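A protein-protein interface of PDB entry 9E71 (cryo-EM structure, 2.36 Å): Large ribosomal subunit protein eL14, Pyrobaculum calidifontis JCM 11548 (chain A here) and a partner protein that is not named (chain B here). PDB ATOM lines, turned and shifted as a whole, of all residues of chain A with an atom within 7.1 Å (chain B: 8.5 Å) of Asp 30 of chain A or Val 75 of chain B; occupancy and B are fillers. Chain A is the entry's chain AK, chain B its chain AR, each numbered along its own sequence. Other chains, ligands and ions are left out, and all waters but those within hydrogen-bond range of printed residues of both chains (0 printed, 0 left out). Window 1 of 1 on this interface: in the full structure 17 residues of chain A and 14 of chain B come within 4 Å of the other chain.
The backbone NH (N) of Lys 3 of chain A is in hydrogen-bond range of the backbone carbonyl oxygen (O) of Arg 77 of chain B (3.0 Å).
O of Ile 5 of chain A is in hydrogen-bond range of N of Val 75 of chain B, at 2.7 Å.
The backbone carbonyl oxygen (O) of Glu 73 of chain B sits at hydrogen-bond distance from the backbone NH (N) of Val 7 of chain A, at 3.2 Å.
The side-chain carboxylate (OD2) of Asp 30 of chain A is in salt-bridge range of the side-chain amino group (NZ) of Lys 32 of chain B (2.7 Å).
ND2 of Asn 32 of chain A sits close to NH2 of Arg 77 of chain B (3.2 Å).
The backbone carbonyl oxygen (O) of Ile 52 of chain A sits at hydrogen-bond distance from the side-chain amino group (NZ) of Lys 3 of chain A (3.5 Å).
The side-chain carboxylate (OD1) of Asp 30 of chain A lies within hydrogen-bond range of the backbone NH (N) of Asn 32 of chain A (2.7 Å).
The backbone NH (N) of Tyr 33 of chain A lies within hydrogen-bond range of the side-chain carboxylate (OD1) of Asp 30 of chain A (2.7 Å).
The side-chain amide nitrogen (ND2) of Asn 51 of chain A sits close to the backbone carbonyl oxygen (O) of Asn 32 of chain A (3.5 Å).
O of Asn 32 of chain A lies within hydrogen-bond range of N of Ile 52 of chain A (2.9 Å).
The backbone carbonyl oxygen (O) of Val 22 of chain B sits at hydrogen-bond distance from the side-chain amino group (NZ) of Lys 32 of chain B (3.0 Å).
Val 75 of chain B touches Lys 3 of chain A.
Val 4 of chain A touches Val 75 of chain B (CA to O, 3.7 Å).
Ile 5 of chain A touches Lys 74 of chain B.
Glu 73 of chain B touches Asp 6 of chain A.
Asp 6 of chain A touches Lys 74 of chain B.
OD2 of Asp 27 of chain A touches CD of Pro 2 of chain B, 3.0 Å away.
Val 29 of chain A touches Glu 24 of chain B (CG1 to OE2, 3.5 Å).
Val 75 of chain B touches Asp 30 of chain A (CG2 to O, 3.7 Å).
OE2 of Glu 31 of chain A touches CD2 of Leu 69 of chain B, 3.1 Å away.
Val 75 of chain B touches Glu 31 of chain A.
Of chain B, only Lys 32 and Val 75 come within 4 Å of Asp 30 of chain A.
Val 75 of chain B touches just these residues of chain A: Lys 3 (3.8 Å), Val 4 (3.7 Å), Ile 5 (2.7 Å), Ile 28 (3.3 Å), Asp 30 (3.7 Å) and Glu 31 (3.0 Å).
Val 29 of chain A touches just these residues of chain B: Val 22 and Glu 24.
Printed residues of chain A within 4 Å of Val 22 of chain B: Val 29 (3.1 Å).
Printed residues of chain A within 4 Å of Glu 24 of chain B: Val 29 (3.5 Å).
Of the printed residues of chain B, Lys 3 of chain A touches Val 75 (3.8 Å), Val 76 (3.3 Å) and Arg 77 (3.0 Å).
Printed residues of chain A within 4 Å of Lys 32 of chain B: Asp 30.
Printed residues of chain B within 4 Å of Val 4 of chain A: Val 75.
Ala 29 of chain B touches none of the printed residues of chain A.
Tyr 33 of chain A touches none of the printed residues of chain B.
Of the 19 printed residues of chain B, 10 touch a printed residue of chain A.
Along chain B the printed residues that touch a printed residue of chain A span positions 2 to 77.
Printed residues of chain A that touch a printed residue of chain B: Lys 3, Val 4, Ile 5, Asp 6, Val 7, Asp 27, Ile 28, Val 29, Asp 30, Glu 31, Asn 32, Asn 51 and Ile 52.
Along chain A the printed residues that touch a printed residue of chain B span positions 3 to 52.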
ATOM      1  N   LYS A   3     -22.787 -14.899  13.849  1.00  0.00           N
ATOM      2  CA  LYS A   3     -21.963 -15.939  13.247  1.00  0.00           C
ATOM      3  C   LYS A   3     -22.594 -16.397  11.941  1.00  0.00           C
ATOM      4  O   LYS A   3     -23.800 -16.660  11.886  1.00  0.00           O
ATOM      5  CB  LYS A   3     -21.797 -17.124  14.198  1.00  0.00           C
ATOM      6  CG  LYS A   3     -21.542 -18.444  13.499  1.00  0.00           C
ATOM      7  CD  LYS A   3     -21.354 -19.569  14.500  1.00  0.00           C
ATOM      8  CE  LYS A   3     -20.284 -19.228  15.519  1.00  0.00           C
ATOM      9  NZ  LYS A   3     -20.498 -19.942  16.807  1.00  0.00           N
ATOM     10  N   VAL A   4     -21.780 -16.489  10.897  1.00  0.00           N
ATOM     11  CA  VAL A   4     -22.238 -16.893   9.576  1.00  0.00           C
ATOM     12  C   VAL A   4     -21.495 -18.159   9.180  1.00  0.00           C
ATOM     13  O   VAL A   4     -20.259 -18.175   9.138  1.00  0.00           O
ATOM     14  CB  VAL A   4     -22.023 -15.786   8.535  1.00  0.00           C
ATOM     15  CG1 VAL A   4     -21.778 -16.393   7.175  1.00  0.00           C
ATOM     16  CG2 VAL A   4     -23.225 -14.863   8.502  1.00  0.00           C
ATOM     17  N   ILE A   5     -22.248 -19.214   8.893  1.00  0.00           N
ATOM     18  CA  ILE A   5     -21.703 -20.481   8.424  1.00  0.00           C
ATOM     19  C   ILE A   5     -22.339 -20.779   7.078  1.00  0.00           C
ATOM     20  O   ILE A   5     -23.569 -20.793   6.958  1.00  0.00           O
ATOM     21  CB  ILE A   5     -21.968 -21.619   9.418  1.00  0.00           C
ATOM     22  CG1 ILE A   5     -21.612 -21.179  10.838  1.00  0.00           C
ATOM     23  CG2 ILE A   5     -21.173 -22.845   9.037  1.00  0.00           C
ATOM     24  CD1 ILE A   5     -20.133 -21.217  11.135  1.00  0.00           C
ATOM     25  N   ASP A   6     -21.505 -21.009   6.067  1.00  0.00           N
ATOM     26  CA  ASP A   6     -21.979 -21.321   4.728  1.00  0.00           C
ATOM     27  C   ASP A   6     -21.121 -22.422   4.123  1.00  0.00           C
ATOM     28  O   ASP A   6     -20.012 -22.692   4.592  1.00  0.00           O
ATOM     29  CB  ASP A   6     -22.010 -20.069   3.831  1.00  0.00           C
ATOM     30  CG  ASP A   6     -20.663 -19.359   3.725  1.00  0.00           C
ATOM     31  OD1 ASP A   6     -20.649 -18.239   3.172  1.00  0.00           O
ATOM     32  OD2 ASP A   6     -19.629 -19.871   4.206  1.00  0.00           O
ATOM     33  N   VAL A   7     -21.651 -23.057   3.077  1.00  0.00           N
ATOM     34  CA  VAL A   7     -20.984 -24.205   2.477  1.00  0.00           C
ATOM     35  C   VAL A   7     -19.683 -23.765   1.824  1.00  0.00           C
ATOM     36  O   VAL A   7     -19.643 -22.784   1.071  1.00  0.00           O
ATOM     37  CB  VAL A   7     -21.912 -24.894   1.467  1.00  0.00           C
ATOM     38  CG1 VAL A   7     -21.112 -25.797   0.555  1.00  0.00           C
ATOM     39  CG2 VAL A   7     -22.982 -25.684   2.190  1.00  0.00           C
ATOM     40  N   ASP A  27     -21.948 -29.317   3.880  1.00  0.00           N
ATOM     41  CA  ASP A  27     -23.387 -29.444   3.728  1.00  0.00           C
ATOM     42  C   ASP A  27     -24.057 -28.928   4.991  1.00  0.00           C
ATOM     43  O   ASP A  27     -23.440 -28.853   6.057  1.00  0.00           O
ATOM     44  CB  ASP A  27     -23.772 -30.897   3.434  1.00  0.00           C
ATOM     45  CG  ASP A  27     -25.184 -31.036   2.909  1.00  0.00           C
ATOM     46  OD1 ASP A  27     -25.939 -30.041   2.930  1.00  0.00           O
ATOM     47  OD2 ASP A  27     -25.528 -32.141   2.445  1.00  0.00           O
ATOM     48  N   ILE A  28     -25.329 -28.565   4.857  1.00  0.00           N
ATOM     49  CA  ILE A  28     -26.119 -28.019   5.953  1.00  0.00           C
ATOM     50  C   ILE A  28     -27.244 -28.994   6.258  1.00  0.00           C
ATOM     51  O   ILE A  28     -28.012 -29.360   5.362  1.00  0.00           O
ATOM     52  CB  ILE A  28     -26.685 -26.632   5.620  1.00  0.00           C
ATOM     53  CG1 ILE A  28     -25.604 -25.746   5.005  1.00  0.00           C
ATOM     54  CG2 ILE A  28     -27.250 -25.987   6.870  1.00  0.00           C
ATOM     55  CD1 ILE A  28     -24.745 -25.049   6.022  1.00  0.00           C
ATOM     56  N   VAL A  29     -27.343 -29.406   7.520  1.00  0.00           N
ATOM     57  CA  VAL A  29     -28.422 -30.294   7.939  1.00  0.00           C
ATOM     58  C   VAL A  29     -29.670 -29.494   8.283  1.00  0.00           C
ATOM     59  O   VAL A  29     -30.766 -29.771   7.785  1.00  0.00           O
ATOM     60  CB  VAL A  29     -27.973 -31.164   9.127  1.00  0.00           C
ATOM     61  CG1 VAL A  29     -29.038 -32.186   9.462  1.00  0.00           C
ATOM     62  CG2 VAL A  29     -26.651 -31.845   8.821  1.00  0.00           C
ATOM     63  N   ASP A  30     -29.521 -28.492   9.142  1.00  0.00           N
ATOM     64  CA  ASP A  30     -30.631 -27.642   9.555  1.00  0.00           C
ATOM     65  C   ASP A  30     -30.057 -26.322  10.053  1.00  0.00           C
ATOM     66  O   ASP A  30     -28.892 -26.001   9.809  1.00  0.00           O
ATOM     67  CB  ASP A  30     -31.497 -28.345  10.610  1.00  0.00           C
ATOM     68  CG  ASP A  30     -30.683 -28.941  11.746  1.00  0.00           C
ATOM     69  OD1 ASP A  30     -29.869 -28.221  12.354  1.00  0.00           O
ATOM     70  OD2 ASP A  30     -30.863 -30.142  12.034  1.00  0.00           O
ATOM     71  N   GLU A  31     -30.881 -25.554  10.770  1.00  0.00           N
ATOM     72  CA  GLU A  31     -30.426 -24.295  11.348  1.00  0.00           C
ATOM     73  C   GLU A  31     -29.390 -24.483  12.446  1.00  0.00           C
ATOM     74  O   GLU A  31     -28.710 -23.516  12.802  1.00  0.00           O
ATOM     75  CB  GLU A  31     -31.613 -23.516  11.911  1.00  0.00           C
ATOM     76  CG  GLU A  31     -32.885 -23.664  11.106  1.00  0.00           C
ATOM     77  CD  GLU A  31     -33.074 -22.545  10.102  1.00  0.00           C
ATOM     78  OE1 GLU A  31     -32.133 -21.746   9.916  1.00  0.00           O
ATOM     79  OE2 GLU A  31     -34.166 -22.461   9.505  1.00  0.00           O
ATOM     80  N   ASN A  32     -29.253 -25.689  12.992  1.00  0.00           N
ATOM     81  CA  ASN A  32     -28.381 -25.939  14.122  1.00  0.00           C
ATOM     82  C   ASN A  32     -27.194 -26.832  13.808  1.00  0.00           C
ATOM     83  O   ASN A  32     -26.228 -26.830  14.577  1.00  0.00           O
ATOM     84  CB  ASN A  32     -29.181 -26.572  15.268  1.00  0.00           C
ATOM     85  CG  ASN A  32     -30.410 -25.773  15.622  1.00  0.00           C
ATOM     86  OD1 ASN A  32     -31.492 -26.324  15.792  1.00  0.00           O
ATOM     87  ND2 ASN A  32     -30.251 -24.462  15.729  1.00  0.00           N
ATOM     88  N   TYR A  33     -27.233 -27.596  12.723  1.00  0.00           N
ATOM     89  CA  TYR A  33     -26.171 -28.531  12.398  1.00  0.00           C
ATOM     90  C   TYR A  33     -25.756 -28.358  10.948  1.00  0.00           C
ATOM     91  O   TYR A  33     -26.575 -28.047  10.083  1.00  0.00           O
ATOM     92  CB  TYR A  33     -26.605 -29.984  12.628  1.00  0.00           C
ATOM     93  CG  TYR A  33     -26.775 -30.361  14.076  1.00  0.00           C
ATOM     94  CD1 TYR A  33     -27.961 -30.107  14.742  1.00  0.00           C
ATOM     95  CD2 TYR A  33     -25.749 -30.975  14.778  1.00  0.00           C
ATOM     96  CE1 TYR A  33     -28.118 -30.448  16.066  1.00  0.00           C
ATOM     97  CE2 TYR A  33     -25.898 -31.320  16.099  1.00  0.00           C
ATOM     98  CZ  TYR A  33     -27.084 -31.053  16.738  1.00  0.00           C
ATOM     99  OH  TYR A  33     -27.246 -31.395  18.056  1.00  0.00           O
ATOM    100  N   VAL A  34     -24.467 -28.569  10.687  1.00  0.00           N
ATOM    101  CA  VAL A  34     -23.939 -28.603   9.332  1.00  0.00           C
ATOM    102  C   VAL A  34     -23.077 -29.849   9.192  1.00  0.00           C
ATOM    103  O   VAL A  34     -22.835 -30.572  10.157  1.00  0.00           O
ATOM    104  CB  VAL A  34     -23.136 -27.339   8.972  1.00  0.00           C
ATOM    105  CG1 VAL A  34     -23.978 -26.104   9.196  1.00  0.00           C
ATOM    106  CG2 VAL A  34     -21.865 -27.269   9.781  1.00  0.00           C
ATOM    107  N   VAL A  50     -21.971 -31.484  12.713  1.00  0.00           N
ATOM    108  CA  VAL A  50     -21.441 -30.669  13.795  1.00  0.00           C
ATOM    109  C   VAL A  50     -22.472 -29.612  14.149  1.00  0.00           C
ATOM    110  O   VAL A  50     -23.164 -29.081  13.276  1.00  0.00           O
ATOM    111  CB  VAL A  50     -20.094 -30.026  13.413  1.00  0.00           C
ATOM    112  CG1 VAL A  50     -20.293 -29.026  12.299  1.00  0.00           C
ATOM    113  CG2 VAL A  50     -19.463 -29.361  14.620  1.00  0.00           C
ATOM    114  N   ASN A  51     -22.579 -29.325  15.441  1.00  0.00           N
ATOM    115  CA  ASN A  51     -23.424 -28.236  15.898  1.00  0.00           C
ATOM    116  C   ASN A  51     -22.777 -26.903  15.556  1.00  0.00           C
ATOM    117  O   ASN A  51     -21.552 -26.781  15.534  1.00  0.00           O
ATOM    118  CB  ASN A  51     -23.658 -28.347  17.403  1.00  0.00           C
ATOM    119  CG  ASN A  51     -24.757 -27.436  17.887  1.00  0.00           C
ATOM    120  OD1 ASN A  51     -24.505 -26.301  18.281  1.00  0.00           O
ATOM    121  ND2 ASN A  51     -25.988 -27.925  17.861  1.00  0.00           N
ATOM    122  N   ILE A  52     -23.612 -25.899  15.285  1.00  0.00           N
ATOM    123  CA  ILE A  52     -23.103 -24.571  14.955  1.00  0.00           C
ATOM    124  C   ILE A  52     -22.369 -23.961  16.138  1.00  0.00           C
ATOM    125  O   ILE A  52     -21.428 -23.180  15.961  1.00  0.00           O
ATOM    126  CB  ILE A  52     -24.249 -23.657  14.484  1.00  0.00           C
ATOM    127  CG1 ILE A  52     -25.030 -24.320  13.355  1.00  0.00           C
ATOM    128  CG2 ILE A  52     -23.705 -22.327  14.021  1.00  0.00           C
ATOM    129  CD1 ILE A  52     -24.213 -24.556  12.127  1.00  0.00           C
ATOM    130  N   PRO B   2     -28.386 -34.685   4.698  1.00  0.00           N
ATOM    131  CA  PRO B   2     -29.720 -34.093   4.837  1.00  0.00           C
ATOM    132  C   PRO B   2     -30.757 -34.794   3.978  1.00  0.00           C
ATOM    133  O   PRO B   2     -30.643 -34.807   2.757  1.00  0.00           O
ATOM    134  CB  PRO B   2     -29.533 -32.642   4.380  1.00  0.00           C
ATOM    135  CG  PRO B   2     -28.202 -32.556   3.779  1.00  0.00           C
ATOM    136  CD  PRO B   2     -27.390 -33.739   4.179  1.00  0.00           C
ATOM    137  N   VAL B  21     -39.253 -34.134   9.130  1.00  0.00           N
ATOM    138  CA  VAL B  21     -38.055 -33.641   9.798  1.00  0.00           C
ATOM    139  C   VAL B  21     -36.865 -33.778   8.863  1.00  0.00           C
ATOM    140  O   VAL B  21     -36.639 -34.849   8.293  1.00  0.00           O
ATOM    141  CB  VAL B  21     -37.792 -34.393  11.115  1.00  0.00           C
ATOM    142  CG1 VAL B  21     -36.435 -34.024  11.663  1.00  0.00           C
ATOM    143  CG2 VAL B  21     -38.872 -34.071  12.121  1.00  0.00           C
ATOM    144  N   VAL B  22     -36.103 -32.702   8.712  1.00  0.00           N
ATOM    145  CA  VAL B  22     -34.860 -32.739   7.952  1.00  0.00           C
ATOM    146  C   VAL B  22     -33.770 -33.286   8.859  1.00  0.00           C
ATOM    147  O   VAL B  22     -33.464 -32.700   9.902  1.00  0.00           O
ATOM    148  CB  VAL B  22     -34.487 -31.352   7.415  1.00  0.00           C
ATOM    149  CG1 VAL B  22     -33.164 -31.414   6.686  1.00  0.00           C
ATOM    150  CG2 VAL B  22     -35.555 -30.859   6.486  1.00  0.00           C
ATOM    151  N   GLY B  23     -33.191 -34.413   8.467  1.00  0.00           N
ATOM    152  CA  GLY B  23     -32.166 -35.049   9.266  1.00  0.00           C
ATOM    153  C   GLY B  23     -31.231 -35.849   8.390  1.00  0.00           C
ATOM    154  O   GLY B  23     -31.622 -36.409   7.362  1.00  0.00           O
ATOM    155  N   GLU B  24     -29.979 -35.897   8.825  1.00  0.00           N
ATOM    156  CA  GLU B  24     -28.950 -36.646   8.118  1.00  0.00           C
ATOM    157  C   GLU B  24     -29.077 -38.146   8.357  1.00  0.00           C
ATOM    158  O   GLU B  24     -28.424 -38.934   7.664  1.00  0.00           O
ATOM    159  CB  GLU B  24     -27.549 -36.137   8.506  1.00  0.00           C
ATOM    160  CG  GLU B  24     -27.082 -36.350   9.959  1.00  0.00           C
ATOM    161  CD  GLU B  24     -27.822 -35.472  10.952  1.00  0.00           C
ATOM    162  OE1 GLU B  24     -28.999 -35.783  11.216  1.00  0.00           O
ATOM    163  OE2 GLU B  24     -27.269 -34.455  11.413  1.00  0.00           O
ATOM    164  N   ASP B  28     -31.284 -39.137  14.065  1.00  0.00           N
ATOM    165  CA  ASP B  28     -31.377 -37.724  14.402  1.00  0.00           C
ATOM    166  C   ASP B  28     -32.759 -37.163  14.122  1.00  0.00           C
ATOM    167  O   ASP B  28     -33.211 -36.248  14.825  1.00  0.00           O
ATOM    168  CB  ASP B  28     -30.321 -36.935  13.652  1.00  0.00           C
ATOM    169  CG  ASP B  28     -28.943 -37.290  14.099  1.00  0.00           C
ATOM    170  OD1 ASP B  28     -28.532 -36.740  15.132  1.00  0.00           O
ATOM    171  OD2 ASP B  28     -28.280 -38.108  13.433  1.00  0.00           O
ATOM    172  N   ALA B  29     -33.444 -37.685  13.100  1.00  0.00           N
ATOM    173  CA  ALA B  29     -34.838 -37.301  12.901  1.00  0.00           C
ATOM    174  C   ALA B  29     -35.685 -37.683  14.109  1.00  0.00           C
ATOM    175  O   ALA B  29     -36.520 -36.894  14.572  1.00  0.00           O
ATOM    176  CB  ALA B  29     -35.389 -37.953  11.637  1.00  0.00           C
ATOM    177  N   LYS B  32     -34.904 -35.391  17.081  1.00  0.00           N
ATOM    178  CA  LYS B  32     -35.619 -34.129  16.899  1.00  0.00           C
ATOM    179  C   LYS B  32     -37.099 -34.272  17.237  1.00  0.00           C
ATOM    180  O   LYS B  32     -37.678 -33.412  17.910  1.00  0.00           O
ATOM    181  CB  LYS B  32     -35.447 -33.637  15.463  1.00  0.00           C
ATOM    182  CG  LYS B  32     -35.481 -32.133  15.317  1.00  0.00           C
ATOM    183  CD  LYS B  32     -34.790 -31.688  14.042  1.00  0.00           C
ATOM    184  CE  LYS B  32     -33.624 -32.596  13.716  1.00  0.00           C
ATOM    185  NZ  LYS B  32     -32.708 -31.991  12.716  1.00  0.00           N
ATOM    186  N   GLU B  65     -41.106 -25.772   5.357  1.00  0.00           N
ATOM    187  CA  GLU B  65     -39.953 -25.501   6.209  1.00  0.00           C
ATOM    188  C   GLU B  65     -38.836 -26.505   5.948  1.00  0.00           C
ATOM    189  O   GLU B  65     -37.673 -26.125   5.780  1.00  0.00           O
ATOM    190  CB  GLU B  65     -40.345 -25.510   7.693  1.00  0.00           C
ATOM    191  CG  GLU B  65     -41.640 -24.781   8.169  1.00  0.00           C
ATOM    192  CD  GLU B  65     -42.113 -23.613   7.304  1.00  0.00           C
ATOM    193  OE1 GLU B  65     -41.263 -22.847   6.807  1.00  0.00           O
ATOM    194  OE2 GLU B  65     -43.340 -23.480   7.119  1.00  0.00           O
ATOM    195  N   ALA B  66     -39.175 -27.794   5.886  1.00  0.00           N
ATOM    196  CA  ALA B  66     -38.167 -28.792   5.552  1.00  0.00           C
ATOM    197  C   ALA B  66     -37.699 -28.637   4.112  1.00  0.00           C
ATOM    198  O   ALA B  66     -36.530 -28.900   3.803  1.00  0.00           O
ATOM    199  CB  ALA B  66     -38.707 -30.198   5.794  1.00  0.00           C
ATOM    200  N   MET B  68     -37.307 -25.770   2.494  1.00  0.00           N
ATOM    201  CA  MET B  68     -36.295 -24.716   2.505  1.00  0.00           C
ATOM    202  C   MET B  68     -35.034 -25.145   3.246  1.00  0.00           C
ATOM    203  O   MET B  68     -33.925 -24.754   2.862  1.00  0.00           O
ATOM    204  CB  MET B  68     -36.859 -23.431   3.106  1.00  0.00           C
ATOM    205  CG  MET B  68     -37.600 -22.530   2.128  1.00  0.00           C
ATOM    206  SD  MET B  68     -39.080 -23.223   1.389  1.00  0.00           S
ATOM    207  CE  MET B  68     -40.327 -22.414   2.380  1.00  0.00           C
ATOM    208  N   LEU B  69     -35.173 -25.935   4.313  1.00  0.00           N
ATOM    209  CA  LEU B  69     -33.985 -26.402   5.021  1.00  0.00           C
ATOM    210  C   LEU B  69     -33.159 -27.345   4.159  1.00  0.00           C
ATOM    211  O   LEU B  69     -31.941 -27.450   4.345  1.00  0.00           O
ATOM    212  CB  LEU B  69     -34.372 -27.088   6.331  1.00  0.00           C
ATOM    213  CG  LEU B  69     -35.086 -26.200   7.345  1.00  0.00           C
ATOM    214  CD1 LEU B  69     -35.535 -26.999   8.552  1.00  0.00           C
ATOM    215  CD2 LEU B  69     -34.195 -25.054   7.757  1.00  0.00           C
ATOM    216  N   MET B  70     -33.805 -28.040   3.221  1.00  0.00           N
ATOM    217  CA  MET B  70     -33.078 -28.890   2.287  1.00  0.00           C
ATOM    218  C   MET B  70     -32.165 -28.078   1.382  1.00  0.00           C
ATOM    219  O   MET B  70     -31.039 -28.499   1.093  1.00  0.00           O
ATOM    220  CB  MET B  70     -34.071 -29.692   1.455  1.00  0.00           C
ATOM    221  CG  MET B  70     -34.541 -30.960   2.124  1.00  0.00           C
ATOM    222  SD  MET B  70     -33.250 -31.819   3.022  1.00  0.00           S
ATOM    223  CE  MET B  70     -33.031 -33.216   1.934  1.00  0.00           C
ATOM    224  N   LEU B  72     -31.124 -24.929   1.985  1.00  0.00           N
ATOM    225  CA  LEU B  72     -30.361 -23.921   2.705  1.00  0.00           C
ATOM    226  C   LEU B  72     -28.885 -24.000   2.337  1.00  0.00           C
ATOM    227  O   LEU B  72     -28.338 -25.085   2.125  1.00  0.00           O
ATOM    228  CB  LEU B  72     -30.533 -24.112   4.211  1.00  0.00           C
ATOM    229  CG  LEU B  72     -30.621 -22.866   5.088  1.00  0.00           C
ATOM    230  CD1 LEU B  72     -31.936 -22.158   4.865  1.00  0.00           C
ATOM    231  CD2 LEU B  72     -30.463 -23.255   6.541  1.00  0.00           C
ATOM    232  N   GLU B  73     -28.241 -22.837   2.246  1.00  0.00           N
ATOM    233  CA  GLU B  73     -26.824 -22.764   1.933  1.00  0.00           C
ATOM    234  C   GLU B  73     -25.992 -22.145   3.045  1.00  0.00           C
ATOM    235  O   GLU B  73     -24.815 -22.493   3.174  1.00  0.00           O
ATOM    236  CB  GLU B  73     -26.604 -21.974   0.634  1.00  0.00           C
ATOM    237  CG  GLU B  73     -25.377 -22.396  -0.168  1.00  0.00           C
ATOM    238  CD  GLU B  73     -24.089 -21.792   0.358  1.00  0.00           C
ATOM    239  OE1 GLU B  73     -24.160 -20.757   1.053  1.00  0.00           O
ATOM    240  OE2 GLU B  73     -23.006 -22.355   0.086  1.00  0.00           O
ATOM    241  N   LYS B  74     -26.561 -21.255   3.852  1.00  0.00           N
ATOM    242  CA  LYS B  74     -25.836 -20.678   4.973  1.00  0.00           C
ATOM    243  C   LYS B  74     -26.779 -20.565   6.158  1.00  0.00           C
ATOM    244  O   LYS B  74     -27.988 -20.397   5.988  1.00  0.00           O
ATOM    245  CB  LYS B  74     -25.259 -19.307   4.620  1.00  0.00           C
ATOM    246  CG  LYS B  74     -26.284 -18.347   4.043  1.00  0.00           C
ATOM    247  CD  LYS B  74     -25.655 -17.014   3.703  1.00  0.00           C
ATOM    248  CE  LYS B  74     -25.321 -16.237   4.963  1.00  0.00           C
ATOM    249  NZ  LYS B  74     -26.534 -15.652   5.590  1.00  0.00           N
ATOM    250  N   VAL B  75     -26.215 -20.650   7.359  1.00  0.00           N
ATOM    251  CA  VAL B  75     -26.987 -20.525   8.586  1.00  0.00           C
ATOM    252  C   VAL B  75     -26.369 -19.427   9.437  1.00  0.00           C
ATOM    253  O   VAL B  75     -25.189 -19.095   9.297  1.00  0.00           O
ATOM    254  CB  VAL B  75     -27.060 -21.853   9.367  1.00  0.00           C
ATOM    255  CG1 VAL B  75     -28.258 -21.854  10.291  1.00  0.00           C
ATOM    256  CG2 VAL B  75     -27.136 -23.022   8.415  1.00  0.00           C
ATOM    257  N   VAL B  76     -27.182 -18.859  10.324  1.00  0.00           N
ATOM    258  CA  VAL B  76     -26.812 -17.687  11.109  1.00  0.00           C
ATOM    259  C   VAL B  76     -27.134 -17.950  12.573  1.00  0.00           C
ATOM    260  O   VAL B  76     -28.153 -18.570  12.893  1.00  0.00           O
ATOM    261  CB  VAL B  76     -27.541 -16.426  10.603  1.00  0.00           C
ATOM    262  CG1 VAL B  76     -27.135 -15.215  11.409  1.00  0.00           C
ATOM    263  CG2 VAL B  76     -27.245 -16.209   9.129  1.00  0.00           C
ATOM    264  N   ARG B  77     -26.259 -17.489  13.461  1.00  0.00           N
ATOM    265  CA  ARG B  77     -26.459 -17.685  14.892  1.00  0.00           C
ATOM    266  C   ARG B  77     -26.076 -16.446  15.690  1.00  0.00           C
ATOM    267  O   ARG B  77     -25.420 -15.544  15.175  1.00  0.00           O
ATOM    268  CB  ARG B  77     -25.658 -18.887  15.380  1.00  0.00           C
ATOM    269  CG  ARG B  77     -26.333 -20.220  15.135  1.00  0.00           C
ATOM    270  CD  ARG B  77     -27.143 -20.656  16.344  1.00  0.00           C
ATOM    271  NE  ARG B  77     -27.001 -22.081  16.617  1.00  0.00           N
ATOM    272  CZ  ARG B  77     -27.868 -22.798  17.317  1.00  0.00           C
ATOM    273  NH1 ARG B  77     -28.959 -22.254  17.829  1.00  0.00           N
ATOM    274  NH2 ARG B  77     -27.632 -24.092  17.513  1.00  0.00           N
